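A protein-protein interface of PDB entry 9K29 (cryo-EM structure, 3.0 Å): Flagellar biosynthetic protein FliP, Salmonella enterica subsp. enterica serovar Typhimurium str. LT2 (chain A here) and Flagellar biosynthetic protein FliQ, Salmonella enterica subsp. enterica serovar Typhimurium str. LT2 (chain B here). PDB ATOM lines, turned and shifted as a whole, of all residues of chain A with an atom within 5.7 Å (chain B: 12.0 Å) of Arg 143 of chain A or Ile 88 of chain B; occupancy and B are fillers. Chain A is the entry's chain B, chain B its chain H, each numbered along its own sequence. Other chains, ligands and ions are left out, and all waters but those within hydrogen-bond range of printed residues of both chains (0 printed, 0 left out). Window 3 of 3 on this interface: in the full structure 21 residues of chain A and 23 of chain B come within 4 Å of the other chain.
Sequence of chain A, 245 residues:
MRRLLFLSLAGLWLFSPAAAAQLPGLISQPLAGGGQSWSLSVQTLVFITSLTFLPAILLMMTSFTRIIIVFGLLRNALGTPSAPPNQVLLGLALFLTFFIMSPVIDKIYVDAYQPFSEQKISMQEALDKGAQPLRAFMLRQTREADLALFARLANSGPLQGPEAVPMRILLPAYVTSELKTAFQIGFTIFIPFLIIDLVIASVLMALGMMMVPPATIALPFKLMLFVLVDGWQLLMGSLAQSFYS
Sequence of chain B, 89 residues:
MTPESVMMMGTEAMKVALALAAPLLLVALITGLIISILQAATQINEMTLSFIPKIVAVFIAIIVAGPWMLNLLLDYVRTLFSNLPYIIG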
ATOM      1  N   ARG A  66       3.441 -15.917   0.671  1.00  0.00           N
ATOM      2  CA  ARG A  66       4.472 -14.929   0.971  1.00  0.00           C
ATOM      3  C   ARG A  66       4.734 -14.846   2.466  1.00  0.00           C
ATOM      4  O   ARG A  66       5.889 -14.851   2.905  1.00  0.00           O
ATOM      5  CB  ARG A  66       4.058 -13.561   0.434  1.00  0.00           C
ATOM      6  CG  ARG A  66       5.122 -12.491   0.593  1.00  0.00           C
ATOM      7  CD  ARG A  66       4.596 -11.120   0.206  1.00  0.00           C
ATOM      8  NE  ARG A  66       4.186 -11.057  -1.191  1.00  0.00           N
ATOM      9  CZ  ARG A  66       3.527 -10.042  -1.730  1.00  0.00           C
ATOM     10  NH1 ARG A  66       3.186  -8.982  -1.016  1.00  0.00           N
ATOM     11  NH2 ARG A  66       3.201 -10.090  -3.019  1.00  0.00           N
ATOM     12  N   GLN A 141      -1.821  -7.899  -7.166  1.00  0.00           N
ATOM     13  CA  GLN A 141      -0.480  -8.287  -6.741  1.00  0.00           C
ATOM     14  C   GLN A 141       0.358  -8.986  -7.805  1.00  0.00           C
ATOM     15  O   GLN A 141       1.541  -9.234  -7.558  1.00  0.00           O
ATOM     16  CB  GLN A 141      -0.539  -9.195  -5.505  1.00  0.00           C
ATOM     17  CG  GLN A 141      -0.722  -8.441  -4.204  1.00  0.00           C
ATOM     18  CD  GLN A 141      -2.161  -8.415  -3.768  1.00  0.00           C
ATOM     19  OE1 GLN A 141      -2.925  -9.314  -4.098  1.00  0.00           O
ATOM     20  NE2 GLN A 141      -2.545  -7.383  -3.030  1.00  0.00           N
ATOM     21  N   THR A 142      -0.204  -9.310  -8.967  1.00  0.00           N
ATOM     22  CA  THR A 142       0.568 -10.021  -9.980  1.00  0.00           C
ATOM     23  C   THR A 142       1.384  -9.044 -10.817  1.00  0.00           C
ATOM     24  O   THR A 142       0.857  -8.043 -11.314  1.00  0.00           O
ATOM     25  CB  THR A 142      -0.350 -10.840 -10.883  1.00  0.00           C
ATOM     26  OG1 THR A 142      -1.195 -11.672 -10.079  1.00  0.00           O
ATOM     27  CG2 THR A 142       0.468 -11.718 -11.815  1.00  0.00           C
ATOM     28  N   ARG A 143       2.672  -9.338 -10.973  1.00  0.00           N
ATOM     29  CA  ARG A 143       3.528  -8.530 -11.829  1.00  0.00           C
ATOM     30  C   ARG A 143       3.208  -8.780 -13.298  1.00  0.00           C
ATOM     31  O   ARG A 143       2.788  -9.872 -13.690  1.00  0.00           O
ATOM     32  CB  ARG A 143       5.000  -8.838 -11.558  1.00  0.00           C
ATOM     33  CG  ARG A 143       5.520  -8.291 -10.241  1.00  0.00           C
ATOM     34  CD  ARG A 143       6.575  -9.208  -9.645  1.00  0.00           C
ATOM     35  NE  ARG A 143       7.419  -8.512  -8.682  1.00  0.00           N
ATOM     36  CZ  ARG A 143       7.841  -9.035  -7.539  1.00  0.00           C
ATOM     37  NH1 ARG A 143       7.507 -10.262  -7.177  1.00  0.00           N
ATOM     38  NH2 ARG A 143       8.615  -8.308  -6.739  1.00  0.00           N
ATOM     39  N   GLU A 144       3.413  -7.746 -14.117  1.00  0.00           N
ATOM     40  CA  GLU A 144       3.139  -7.871 -15.544  1.00  0.00           C
ATOM     41  C   GLU A 144       4.117  -8.817 -16.228  1.00  0.00           C
ATOM     42  O   GLU A 144       3.770  -9.442 -17.237  1.00  0.00           O
ATOM     43  CB  GLU A 144       3.182  -6.495 -16.210  1.00  0.00           C
ATOM     44  CG  GLU A 144       2.079  -5.552 -15.759  1.00  0.00           C
ATOM     45  CD  GLU A 144       0.702  -6.018 -16.188  1.00  0.00           C
ATOM     46  OE1 GLU A 144       0.593  -6.651 -17.259  1.00  0.00           O
ATOM     47  OE2 GLU A 144      -0.273  -5.751 -15.454  1.00  0.00           O
ATOM     48  N   ALA A 145       5.340  -8.929 -15.702  1.00  0.00           N
ATOM     49  CA  ALA A 145       6.335  -9.804 -16.313  1.00  0.00           C
ATOM     50  C   ALA A 145       5.889 -11.259 -16.270  1.00  0.00           C
ATOM     51  O   ALA A 145       6.036 -11.995 -17.251  1.00  0.00           O
ATOM     52  CB  ALA A 145       7.684  -9.630 -15.616  1.00  0.00           C
ATOM     53  N   ASP A 146       5.340 -11.695 -15.133  1.00  0.00           N
ATOM     54  CA  ASP A 146       4.866 -13.072 -15.019  1.00  0.00           C
ATOM     55  C   ASP A 146       3.691 -13.333 -15.953  1.00  0.00           C
ATOM     56  O   ASP A 146       3.614 -14.395 -16.584  1.00  0.00           O
ATOM     57  CB  ASP A 146       4.477 -13.369 -13.573  1.00  0.00           C
ATOM     58  CG  ASP A 146       5.673 -13.407 -12.648  1.00  0.00           C
ATOM     59  OD1 ASP A 146       6.775 -13.755 -13.117  1.00  0.00           O
ATOM     60  OD2 ASP A 146       5.513 -13.087 -11.453  1.00  0.00           O
ATOM     61  N   LEU A 147       2.764 -12.378 -16.046  1.00  0.00           N
ATOM     62  CA  LEU A 147       1.632 -12.530 -16.953  1.00  0.00           C
ATOM     63  C   LEU A 147       2.106 -12.646 -18.394  1.00  0.00           C
ATOM     64  O   LEU A 147       1.622 -13.494 -19.151  1.00  0.00           O
ATOM     65  CB  LEU A 147       0.670 -11.353 -16.793  1.00  0.00           C
ATOM     66  CG  LEU A 147      -0.104 -11.282 -15.477  1.00  0.00           C
ATOM     67  CD1 LEU A 147      -1.027 -10.075 -15.464  1.00  0.00           C
ATOM     68  CD2 LEU A 147      -0.892 -12.561 -15.258  1.00  0.00           C
ATOM     69  N   ALA A 148       3.064 -11.805 -18.788  1.00  0.00           N
ATOM     70  CA  ALA A 148       3.606 -11.885 -20.140  1.00  0.00           C
ATOM     71  C   ALA A 148       4.309 -13.216 -20.374  1.00  0.00           C
ATOM     72  O   ALA A 148       4.159 -13.827 -21.439  1.00  0.00           O
ATOM     73  CB  ALA A 148       4.563 -10.721 -20.392  1.00  0.00           C
ATOM     74  N   ALA A 173       1.137 -17.307 -12.560  1.00  0.00           N
ATOM     75  CA  ALA A 173       1.830 -16.023 -12.532  1.00  0.00           C
ATOM     76  C   ALA A 173       1.753 -15.389 -11.151  1.00  0.00           C
ATOM     77  O   ALA A 173       2.750 -14.854 -10.647  1.00  0.00           O
ATOM     78  CB  ALA A 173       1.242 -15.087 -13.588  1.00  0.00           C
ATOM     79  N   THR A 176       4.134 -17.292  -8.885  1.00  0.00           N
ATOM     80  CA  THR A 176       5.526 -16.939  -9.149  1.00  0.00           C
ATOM     81  C   THR A 176       5.865 -15.568  -8.576  1.00  0.00           C
ATOM     82  O   THR A 176       6.933 -15.384  -7.977  1.00  0.00           O
ATOM     83  CB  THR A 176       5.798 -16.974 -10.652  1.00  0.00           C
ATOM     84  OG1 THR A 176       5.524 -18.287 -11.157  1.00  0.00           O
ATOM     85  CG2 THR A 176       7.248 -16.622 -10.941  1.00  0.00           C
ATOM     86  N   SER A 177       4.967 -14.596  -8.746  1.00  0.00           N
ATOM     87  CA  SER A 177       5.211 -13.268  -8.193  1.00  0.00           C
ATOM     88  C   SER A 177       5.292 -13.311  -6.672  1.00  0.00           C
ATOM     89  O   SER A 177       6.157 -12.662  -6.072  1.00  0.00           O
ATOM     90  CB  SER A 177       4.119 -12.299  -8.644  1.00  0.00           C
ATOM     91  OG  SER A 177       2.835 -12.871  -8.484  1.00  0.00           O
ATOM     92  N   GLU A 178       4.401 -14.073  -6.032  1.00  0.00           N
ATOM     93  CA  GLU A 178       4.443 -14.184  -4.577  1.00  0.00           C
ATOM     94  C   GLU A 178       5.729 -14.852  -4.108  1.00  0.00           C
ATOM     95  O   GLU A 178       6.326 -14.427  -3.113  1.00  0.00           O
ATOM     96  CB  GLU A 178       3.223 -14.947  -4.066  1.00  0.00           C
ATOM     97  CG  GLU A 178       1.915 -14.217  -4.287  1.00  0.00           C
ATOM     98  CD  GLU A 178       1.818 -12.947  -3.465  1.00  0.00           C
ATOM     99  OE1 GLU A 178       2.387 -12.913  -2.354  1.00  0.00           O
ATOM    100  OE2 GLU A 178       1.180 -11.981  -3.931  1.00  0.00           O
ATOM    101  N   LYS A 180       8.657 -14.851  -5.662  1.00  0.00           N
ATOM    102  CA  LYS A 180       9.754 -13.911  -5.859  1.00  0.00           C
ATOM    103  C   LYS A 180       9.747 -12.827  -4.787  1.00  0.00           C
ATOM    104  O   LYS A 180      10.795 -12.478  -4.232  1.00  0.00           O
ATOM    105  CB  LYS A 180       9.667 -13.297  -7.257  1.00  0.00           C
ATOM    106  CG  LYS A 180      10.812 -12.365  -7.605  1.00  0.00           C
ATOM    107  CD  LYS A 180      10.678 -11.842  -9.025  1.00  0.00           C
ATOM    108  CE  LYS A 180      11.870 -10.983  -9.412  1.00  0.00           C
ATOM    109  NZ  LYS A 180      11.914  -9.714  -8.636  1.00  0.00           N
ATOM    110  N   THR A 181       8.564 -12.293  -4.472  1.00  0.00           N
ATOM    111  CA  THR A 181       8.470 -11.251  -3.454  1.00  0.00           C
ATOM    112  C   THR A 181       8.863 -11.780  -2.080  1.00  0.00           C
ATOM    113  O   THR A 181       9.564 -11.100  -1.320  1.00  0.00           O
ATOM    114  CB  THR A 181       7.053 -10.680  -3.423  1.00  0.00           C
ATOM    115  OG1 THR A 181       6.710 -10.184  -4.722  1.00  0.00           O
ATOM    116  CG2 THR A 181       6.959  -9.550  -2.418  1.00  0.00           C
ATOM    117  N   GLN A 184      12.596 -12.106  -1.960  1.00  0.00           N
ATOM    118  CA  GLN A 184      13.203 -10.785  -1.819  1.00  0.00           C
ATOM    119  C   GLN A 184      13.130 -10.298  -0.377  1.00  0.00           C
ATOM    120  O   GLN A 184      14.122  -9.817   0.186  1.00  0.00           O
ATOM    121  CB  GLN A 184      12.509  -9.793  -2.750  1.00  0.00           C
ATOM    122  CG  GLN A 184      12.809  -9.989  -4.221  1.00  0.00           C
ATOM    123  CD  GLN A 184      12.424  -8.784  -5.051  1.00  0.00           C
ATOM    124  OE1 GLN A 184      11.908  -8.917  -6.159  1.00  0.00           O
ATOM    125  NE2 GLN A 184      12.663  -7.595  -4.510  1.00  0.00           N
ATOM    126  N   ILE A 185      11.950 -10.418   0.238  1.00  0.00           N
ATOM    127  CA  ILE A 185      11.775  -9.954   1.611  1.00  0.00           C
ATOM    128  C   ILE A 185      12.653 -10.756   2.560  1.00  0.00           C
ATOM    129  O   ILE A 185      13.286 -10.198   3.466  1.00  0.00           O
ATOM    130  CB  ILE A 185      10.290 -10.021   2.012  1.00  0.00           C
ATOM    131  CG1 ILE A 185       9.472  -9.028   1.187  1.00  0.00           C
ATOM    132  CG2 ILE A 185      10.125  -9.730   3.493  1.00  0.00           C
ATOM    133  CD1 ILE A 185       7.987  -9.094   1.452  1.00  0.00           C
ATOM    134  N   THR A 188      16.273  -9.644   2.213  1.00  0.00           N
ATOM    135  CA  THR A 188      16.454  -8.383   2.925  1.00  0.00           C
ATOM    136  C   THR A 188      16.478  -8.597   4.434  1.00  0.00           C
ATOM    137  O   THR A 188      17.201  -7.894   5.150  1.00  0.00           O
ATOM    138  CB  THR A 188      15.350  -7.399   2.540  1.00  0.00           C
ATOM    139  OG1 THR A 188      15.341  -7.225   1.118  1.00  0.00           O
ATOM    140  CG2 THR A 188      15.584  -6.049   3.195  1.00  0.00           C
ATOM    141  N   SER A 242       2.767  -4.511   1.928  1.00  0.00           N
ATOM    142  CA  SER A 242       3.306  -5.028   0.680  1.00  0.00           C
ATOM    143  C   SER A 242       2.244  -5.640  -0.222  1.00  0.00           C
ATOM    144  O   SER A 242       2.554  -5.979  -1.369  1.00  0.00           O
ATOM    145  CB  SER A 242       4.391  -6.067   0.973  1.00  0.00           C
ATOM    146  OG  SER A 242       3.825  -7.347   1.185  1.00  0.00           O
ATOM    147  N   MET B   1      13.837  -5.566  -8.730  1.00  0.00           N
ATOM    148  CA  MET B   1      14.978  -5.464  -7.829  1.00  0.00           C
ATOM    149  C   MET B   1      16.264  -5.669  -8.622  1.00  0.00           C
ATOM    150  O   MET B   1      16.782  -6.782  -8.720  1.00  0.00           O
ATOM    151  CB  MET B   1      14.855  -6.485  -6.696  1.00  0.00           C
ATOM    152  CG  MET B   1      15.947  -6.420  -5.641  1.00  0.00           C
ATOM    153  SD  MET B   1      15.632  -7.605  -4.318  1.00  0.00           S
ATOM    154  CE  MET B   1      17.085  -7.395  -3.295  1.00  0.00           C
ATOM    155  N   THR B   2      16.767  -4.577  -9.194  1.00  0.00           N
ATOM    156  CA  THR B   2      17.904  -4.649 -10.094  1.00  0.00           C
ATOM    157  C   THR B   2      19.176  -5.024  -9.333  1.00  0.00           C
ATOM    158  O   THR B   2      19.279  -4.791  -8.126  1.00  0.00           O
ATOM    159  CB  THR B   2      18.105  -3.313 -10.804  1.00  0.00           C
ATOM    160  OG1 THR B   2      18.374  -2.292  -9.836  1.00  0.00           O
ATOM    161  CG2 THR B   2      16.859  -2.938 -11.593  1.00  0.00           C
ATOM    162  N   PRO B   3      20.156  -5.619 -10.018  1.00  0.00           N
ATOM    163  CA  PRO B   3      21.435  -5.920  -9.353  1.00  0.00           C
ATOM    164  C   PRO B   3      22.152  -4.693  -8.823  1.00  0.00           C
ATOM    165  O   PRO B   3      22.932  -4.818  -7.873  1.00  0.00           O
ATOM    166  CB  PRO B   3      22.252  -6.619 -10.450  1.00  0.00           C
ATOM    167  CG  PRO B   3      21.555  -6.296 -11.735  1.00  0.00           C
ATOM    168  CD  PRO B   3      20.110  -6.147 -11.390  1.00  0.00           C
ATOM    169  N   SER B   5      20.700  -2.164  -7.274  1.00  0.00           N
ATOM    170  CA  SER B   5      20.132  -1.989  -5.942  1.00  0.00           C
ATOM    171  C   SER B   5      20.733  -2.986  -4.962  1.00  0.00           C
ATOM    172  O   SER B   5      21.043  -2.635  -3.816  1.00  0.00           O
ATOM    173  CB  SER B   5      18.612  -2.136  -5.995  1.00  0.00           C
ATOM    174  OG  SER B   5      18.029  -1.870  -4.731  1.00  0.00           O
ATOM    175  N   VAL B   6      20.918  -4.232  -5.401  1.00  0.00           N
ATOM    176  CA  VAL B   6      21.529  -5.240  -4.541  1.00  0.00           C
ATOM    177  C   VAL B   6      22.949  -4.832  -4.175  1.00  0.00           C
ATOM    178  O   VAL B   6      23.367  -4.963  -3.022  1.00  0.00           O
ATOM    179  CB  VAL B   6      21.492  -6.620  -5.223  1.00  0.00           C
ATOM    180  CG1 VAL B   6      22.441  -7.584  -4.531  1.00  0.00           C
ATOM    181  CG2 VAL B   6      20.081  -7.168  -5.223  1.00  0.00           C
ATOM    182  N   MET B   8      24.300  -1.711  -4.106  1.00  0.00           N
ATOM    183  CA  MET B   8      24.341  -0.573  -3.189  1.00  0.00           C
ATOM    184  C   MET B   8      23.909  -0.986  -1.784  1.00  0.00           C
ATOM    185  O   MET B   8      24.524  -0.573  -0.791  1.00  0.00           O
ATOM    186  CB  MET B   8      23.498   0.587  -3.729  1.00  0.00           C
ATOM    187  CG  MET B   8      22.013   0.321  -3.923  1.00  0.00           C
ATOM    188  SD  MET B   8      21.038   0.400  -2.407  1.00  0.00           S
ATOM    189  CE  MET B   8      21.087   2.161  -2.078  1.00  0.00           C
ATOM    190  N   MET B   9      22.872  -1.822  -1.685  1.00  0.00           N
ATOM    191  CA  MET B   9      22.441  -2.327  -0.386  1.00  0.00           C
ATOM    192  C   MET B   9      23.540  -3.147   0.280  1.00  0.00           C
ATOM    193  O   MET B   9      23.781  -3.018   1.486  1.00  0.00           O
ATOM    194  CB  MET B   9      21.169  -3.156  -0.565  1.00  0.00           C
ATOM    195  CG  MET B   9      20.685  -3.881   0.671  1.00  0.00           C
ATOM    196  SD  MET B   9      19.476  -5.148   0.238  1.00  0.00           S
ATOM    197  CE  MET B   9      18.327  -4.207  -0.763  1.00  0.00           C
ATOM    198  N   THR B  79      15.697   1.603   9.220  1.00  0.00           N
ATOM    199  CA  THR B  79      15.616   2.054   7.835  1.00  0.00           C
ATOM    200  C   THR B  79      15.340   0.888   6.893  1.00  0.00           C
ATOM    201  O   THR B  79      14.514   1.000   5.978  1.00  0.00           O
ATOM    202  CB  THR B  79      16.908   2.770   7.440  1.00  0.00           C
ATOM    203  OG1 THR B  79      17.102   3.909   8.287  1.00  0.00           O
ATOM    204  CG2 THR B  79      16.842   3.230   5.994  1.00  0.00           C
ATOM    205  N   LEU B  80      16.014  -0.243   7.112  1.00  0.00           N
ATOM    206  CA  LEU B  80      15.810  -1.403   6.252  1.00  0.00           C
ATOM    207  C   LEU B  80      14.378  -1.919   6.344  1.00  0.00           C
ATOM    208  O   LEU B  80      13.745  -2.202   5.321  1.00  0.00           O
ATOM    209  CB  LEU B  80      16.803  -2.504   6.619  1.00  0.00           C
ATOM    210  CG  LEU B  80      17.047  -3.584   5.567  1.00  0.00           C
ATOM    211  CD1 LEU B  80      17.780  -3.002   4.370  1.00  0.00           C
ATOM    212  CD2 LEU B  80      17.828  -4.738   6.166  1.00  0.00           C
ATOM    213  N   PHE B  81      13.841  -2.027   7.561  1.00  0.00           N
ATOM    214  CA  PHE B  81      12.488  -2.549   7.715  1.00  0.00           C
ATOM    215  C   PHE B  81      11.440  -1.543   7.256  1.00  0.00           C
ATOM    216  O   PHE B  81      10.330  -1.937   6.884  1.00  0.00           O
ATOM    217  CB  PHE B  81      12.243  -2.956   9.167  1.00  0.00           C
ATOM    218  CG  PHE B  81      12.901  -4.252   9.552  1.00  0.00           C
ATOM    219  CD1 PHE B  81      13.633  -4.977   8.628  1.00  0.00           C
ATOM    220  CD2 PHE B  81      12.788  -4.745  10.841  1.00  0.00           C
ATOM    221  CE1 PHE B  81      14.239  -6.167   8.980  1.00  0.00           C
ATOM    222  CE2 PHE B  81      13.391  -5.936  11.198  1.00  0.00           C
ATOM    223  CZ  PHE B  81      14.118  -6.647  10.266  1.00  0.00           C
ATOM    224  N   SER B  82      11.765  -0.248   7.276  1.00  0.00           N
ATOM    225  CA  SER B  82      10.834   0.748   6.762  1.00  0.00           C
ATOM    226  C   SER B  82      10.821   0.755   5.238  1.00  0.00           C
ATOM    227  O   SER B  82       9.774   0.987   4.624  1.00  0.00           O
ATOM    228  CB  SER B  82      11.192   2.130   7.305  1.00  0.00           C
ATOM    229  OG  SER B  82      10.827   2.251   8.669  1.00  0.00           O
ATOM    230  N   ASN B  83      11.970   0.513   4.614  1.00  0.00           N
ATOM    231  CA  ASN B  83      12.053   0.446   3.160  1.00  0.00           C
ATOM    232  C   ASN B  83      11.710  -0.933   2.611  1.00  0.00           C
ATOM    233  O   ASN B  83      11.647  -1.097   1.388  1.00  0.00           O
ATOM    234  CB  ASN B  83      13.452   0.856   2.693  1.00  0.00           C
ATOM    235  CG  ASN B  83      13.809   2.270   3.102  1.00  0.00           C
ATOM    236  OD1 ASN B  83      13.089   2.906   3.872  1.00  0.00           O
ATOM    237  ND2 ASN B  83      14.927   2.770   2.589  1.00  0.00           N
ATOM    238  N   LEU B  84      11.507  -1.921   3.481  1.00  0.00           N
ATOM    239  CA  LEU B  84      11.106  -3.253   3.027  1.00  0.00           C
ATOM    240  C   LEU B  84       9.878  -3.252   2.125  1.00  0.00           C
ATOM    241  O   LEU B  84       9.920  -3.908   1.069  1.00  0.00           O
ATOM    242  CB  LEU B  84      10.896  -4.159   4.245  1.00  0.00           C
ATOM    243  CG  LEU B  84      10.717  -5.652   3.973  1.00  0.00           C
ATOM    244  CD1 LEU B  84      11.945  -6.221   3.295  1.00  0.00           C
ATOM    245  CD2 LEU B  84      10.424  -6.393   5.266  1.00  0.00           C
ATOM    246  N   PRO B  85       8.764  -2.565   2.450  1.00  0.00           N
ATOM    247  CA  PRO B  85       7.589  -2.650   1.569  1.00  0.00           C
ATOM    248  C   PRO B  85       7.701  -1.785   0.322  1.00  0.00           C
ATOM    249  O   PRO B  85       6.736  -1.666  -0.437  1.00  0.00           O
ATOM    250  CB  PRO B  85       6.446  -2.176   2.472  1.00  0.00           C
ATOM    251  CG  PRO B  85       7.093  -1.228   3.399  1.00  0.00           C
ATOM    252  CD  PRO B  85       8.463  -1.790   3.668  1.00  0.00           C
ATOM    253  N   TYR B  86       8.865  -1.180   0.099  1.00  0.00           N
ATOM    254  CA  TYR B  86       9.080  -0.326  -1.061  1.00  0.00           C
ATOM    255  C   TYR B  86      10.182  -0.810  -1.989  1.00  0.00           C
ATOM    256  O   TYR B  86      10.108  -0.549  -3.192  1.00  0.00           O
ATOM    257  CB  TYR B  86       9.400   1.109  -0.616  1.00  0.00           C
ATOM    258  CG  TYR B  86       8.296   1.750   0.192  1.00  0.00           C
ATOM    259  CD1 TYR B  86       6.964   1.572  -0.155  1.00  0.00           C
ATOM    260  CD2 TYR B  86       8.585   2.531   1.302  1.00  0.00           C
ATOM    261  CE1 TYR B  86       5.950   2.154   0.579  1.00  0.00           C
ATOM    262  CE2 TYR B  86       7.577   3.117   2.044  1.00  0.00           C
ATOM    263  CZ  TYR B  86       6.262   2.926   1.678  1.00  0.00           C
ATOM    264  OH  TYR B  86       5.254   3.507   2.412  1.00  0.00           O
ATOM    265  N   ILE B  87      11.198  -1.503  -1.472  1.00  0.00           N
ATOM    266  CA  ILE B  87      12.256  -2.020  -2.334  1.00  0.00           C
ATOM    267  C   ILE B  87      11.804  -3.235  -3.132  1.00  0.00           C
ATOM    268  O   ILE B  87      12.470  -3.611  -4.104  1.00  0.00           O
ATOM    269  CB  ILE B  87      13.507  -2.375  -1.515  1.00  0.00           C
ATOM    270  CG1 ILE B  87      13.185  -3.472  -0.499  1.00  0.00           C
ATOM    271  CG2 ILE B  87      14.060  -1.140  -0.821  1.00  0.00           C
ATOM    272  CD1 ILE B  87      14.406  -4.058   0.174  1.00  0.00           C
ATOM    273  N   ILE B  88      10.688  -3.862  -2.747  1.00  0.00           N
ATOM    274  CA  ILE B  88      10.203  -5.052  -3.439  1.00  0.00           C
ATOM    275  C   ILE B  88       9.255  -4.731  -4.584  1.00  0.00           C
ATOM    276  O   ILE B  88       8.927  -5.630  -5.373  1.00  0.00           O
ATOM    277  CB  ILE B  88       9.498  -6.000  -2.450  1.00  0.00           C
ATOM    278  CG1 ILE B  88       8.260  -5.322  -1.863  1.00  0.00           C
ATOM    279  CG2 ILE B  88      10.453  -6.420  -1.345  1.00  0.00           C
ATOM    280  CD1 ILE B  88       7.401  -6.237  -1.031  1.00  0.00           C
ATOM    281  N   GLY B  89       8.806  -3.487  -4.705  1.00  0.00           N
ATOM    282  CA  GLY B  89       7.897  -3.107  -5.771  1.00  0.00           C
ATOM    283  C   GLY B  89       6.636  -2.431  -5.271  1.00  0.00           C
ATOM    284  O   GLY B  89       6.343  -2.440  -4.076  1.00  0.00           O
ATOM    285  OXT GLY B  89       5.874  -1.857  -6.049  1.00  0.00           O
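The side-chain amide nitrogen of Gln 184 of chain A is in hydrogen-bond range of the side-chain sulfur of Met 1 of chain B. The backbone carbonyl oxygen (O) of Ile 88 of chain B lies within hydrogen-bond range of the guanidinium group (NH2) of Arg 143 of chain A, 3.0 Å away.
NH1 of Arg 143 of chain A is in hydrogen-bond range of O of Ser 177 of chain A, 3.0 Å away. The guanidinium group of Arg 143 of chain A lies within hydrogen-bond range of the side-chain hydroxyl of Thr 181 of chain A (2.6 Å). OG1 of Thr 188 of chain A sits at hydrogen-bond distance from O of Gln 184 of chain A (3.0 Å). The guanidinium group of Arg 143 of chain A lies within hydrogen-bond range of the side-chain amide oxygen of Gln 184 of chain A. The backbone carbonyl oxygen (O) of Ser 177 of chain A lies within hydrogen-bond range of the side-chain hydroxyl (OG1) of Thr 181 of chain A (2.9 Å). OG of Ser 242 of chain A is in hydrogen-bond range of NH1 of Arg 66 of chain A.
Among the printed residues, pairs that only touch across the chains: Thr 188 of chain A with Leu 80 of chain B (3.4 Å), Thr 188 of chain A with Ile 87 of chain B (3.4 Å), Thr 181 of chain A with Ile 88 of chain B (3.6 Å), Ser 242 of chain A with Ile 88 of chain B (3.6 Å), Thr 188 of chain A with Leu 84 of chain B (3.6 Å), Gln 184 of chain A with Ile 88 of chain B (3.7 Å), Ile 185 of chain A with Ile 88 of chain B (3.8 Å) and Ile 185 of chain A with Leu 84 of chain B (3.8 Å).
No residue of chain B comes within 4 Å of Thr 142 of chain A. Printed residues of chain B within 4 Å of Arg 143 of chain A: Ile 88. No residue of chain B comes within 4 Å of Glu 144 of chain A. No residue of chain B comes within 4 Å of Ala 145 of chain A. No residue of chain B comes within 4 Å of Asp 146 of chain A. No residue of chain B comes within 4 Å of Leu 147 of chain A. No residue of chain B comes within 4 Å of Ser 177 of chain A. No residue of chain B comes within 4 Å of Lys 180 of chain A. Of the printed residues of chain B, Gln 184 of chain A touches Met 1 (3.0 Å) and Ile 88 (3.7 Å). Of the printed residues of chain B, Thr 188 of chain A touches Leu 80 (3.4 Å), Leu 84 (3.6 Å) and Ile 87 (3.4 Å). Ser 5 of chain B touches none of the printed residues of chain A. Val 6 of chain B touches none of the printed residues of chain A. Printed residues of chain A within 4 Å of Leu 80 of chain B: Thr 188 (3.4 Å). Printed residues of chain A within 4 Å of Leu 84 of chain B: Ile 185 and Thr 188. Of the printed residues of chain A, Ile 87 of chain B touches Thr 188. Ile 88 of chain B touches just these residues of chain A: Arg 143 (3.0 Å), Thr 181 (3.6 Å), Gln 184 (3.7 Å), Ile 185 (3.8 Å) and Ser 242 (3.6 Å). The nearest residue of chain A that does not touch Ile 88 of chain B is Arg 66 of chain A (5.0 Å). The nearest printed residue of chain B that does not touch Gln 184 of chain A is Ile 87 of chain B (4.01 Å).
Of the 19 printed residues of chain A, 6 touch a printed residue of chain B. Printed residues of chain A that touch a printed residue of chain B: Arg 143, Thr 181, Gln 184, Ile 185, Thr 188 and Ser 242. Hydrophobic or aromatic side chains of chain A within 4 Å of the printed part of chain B: Ile 185.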
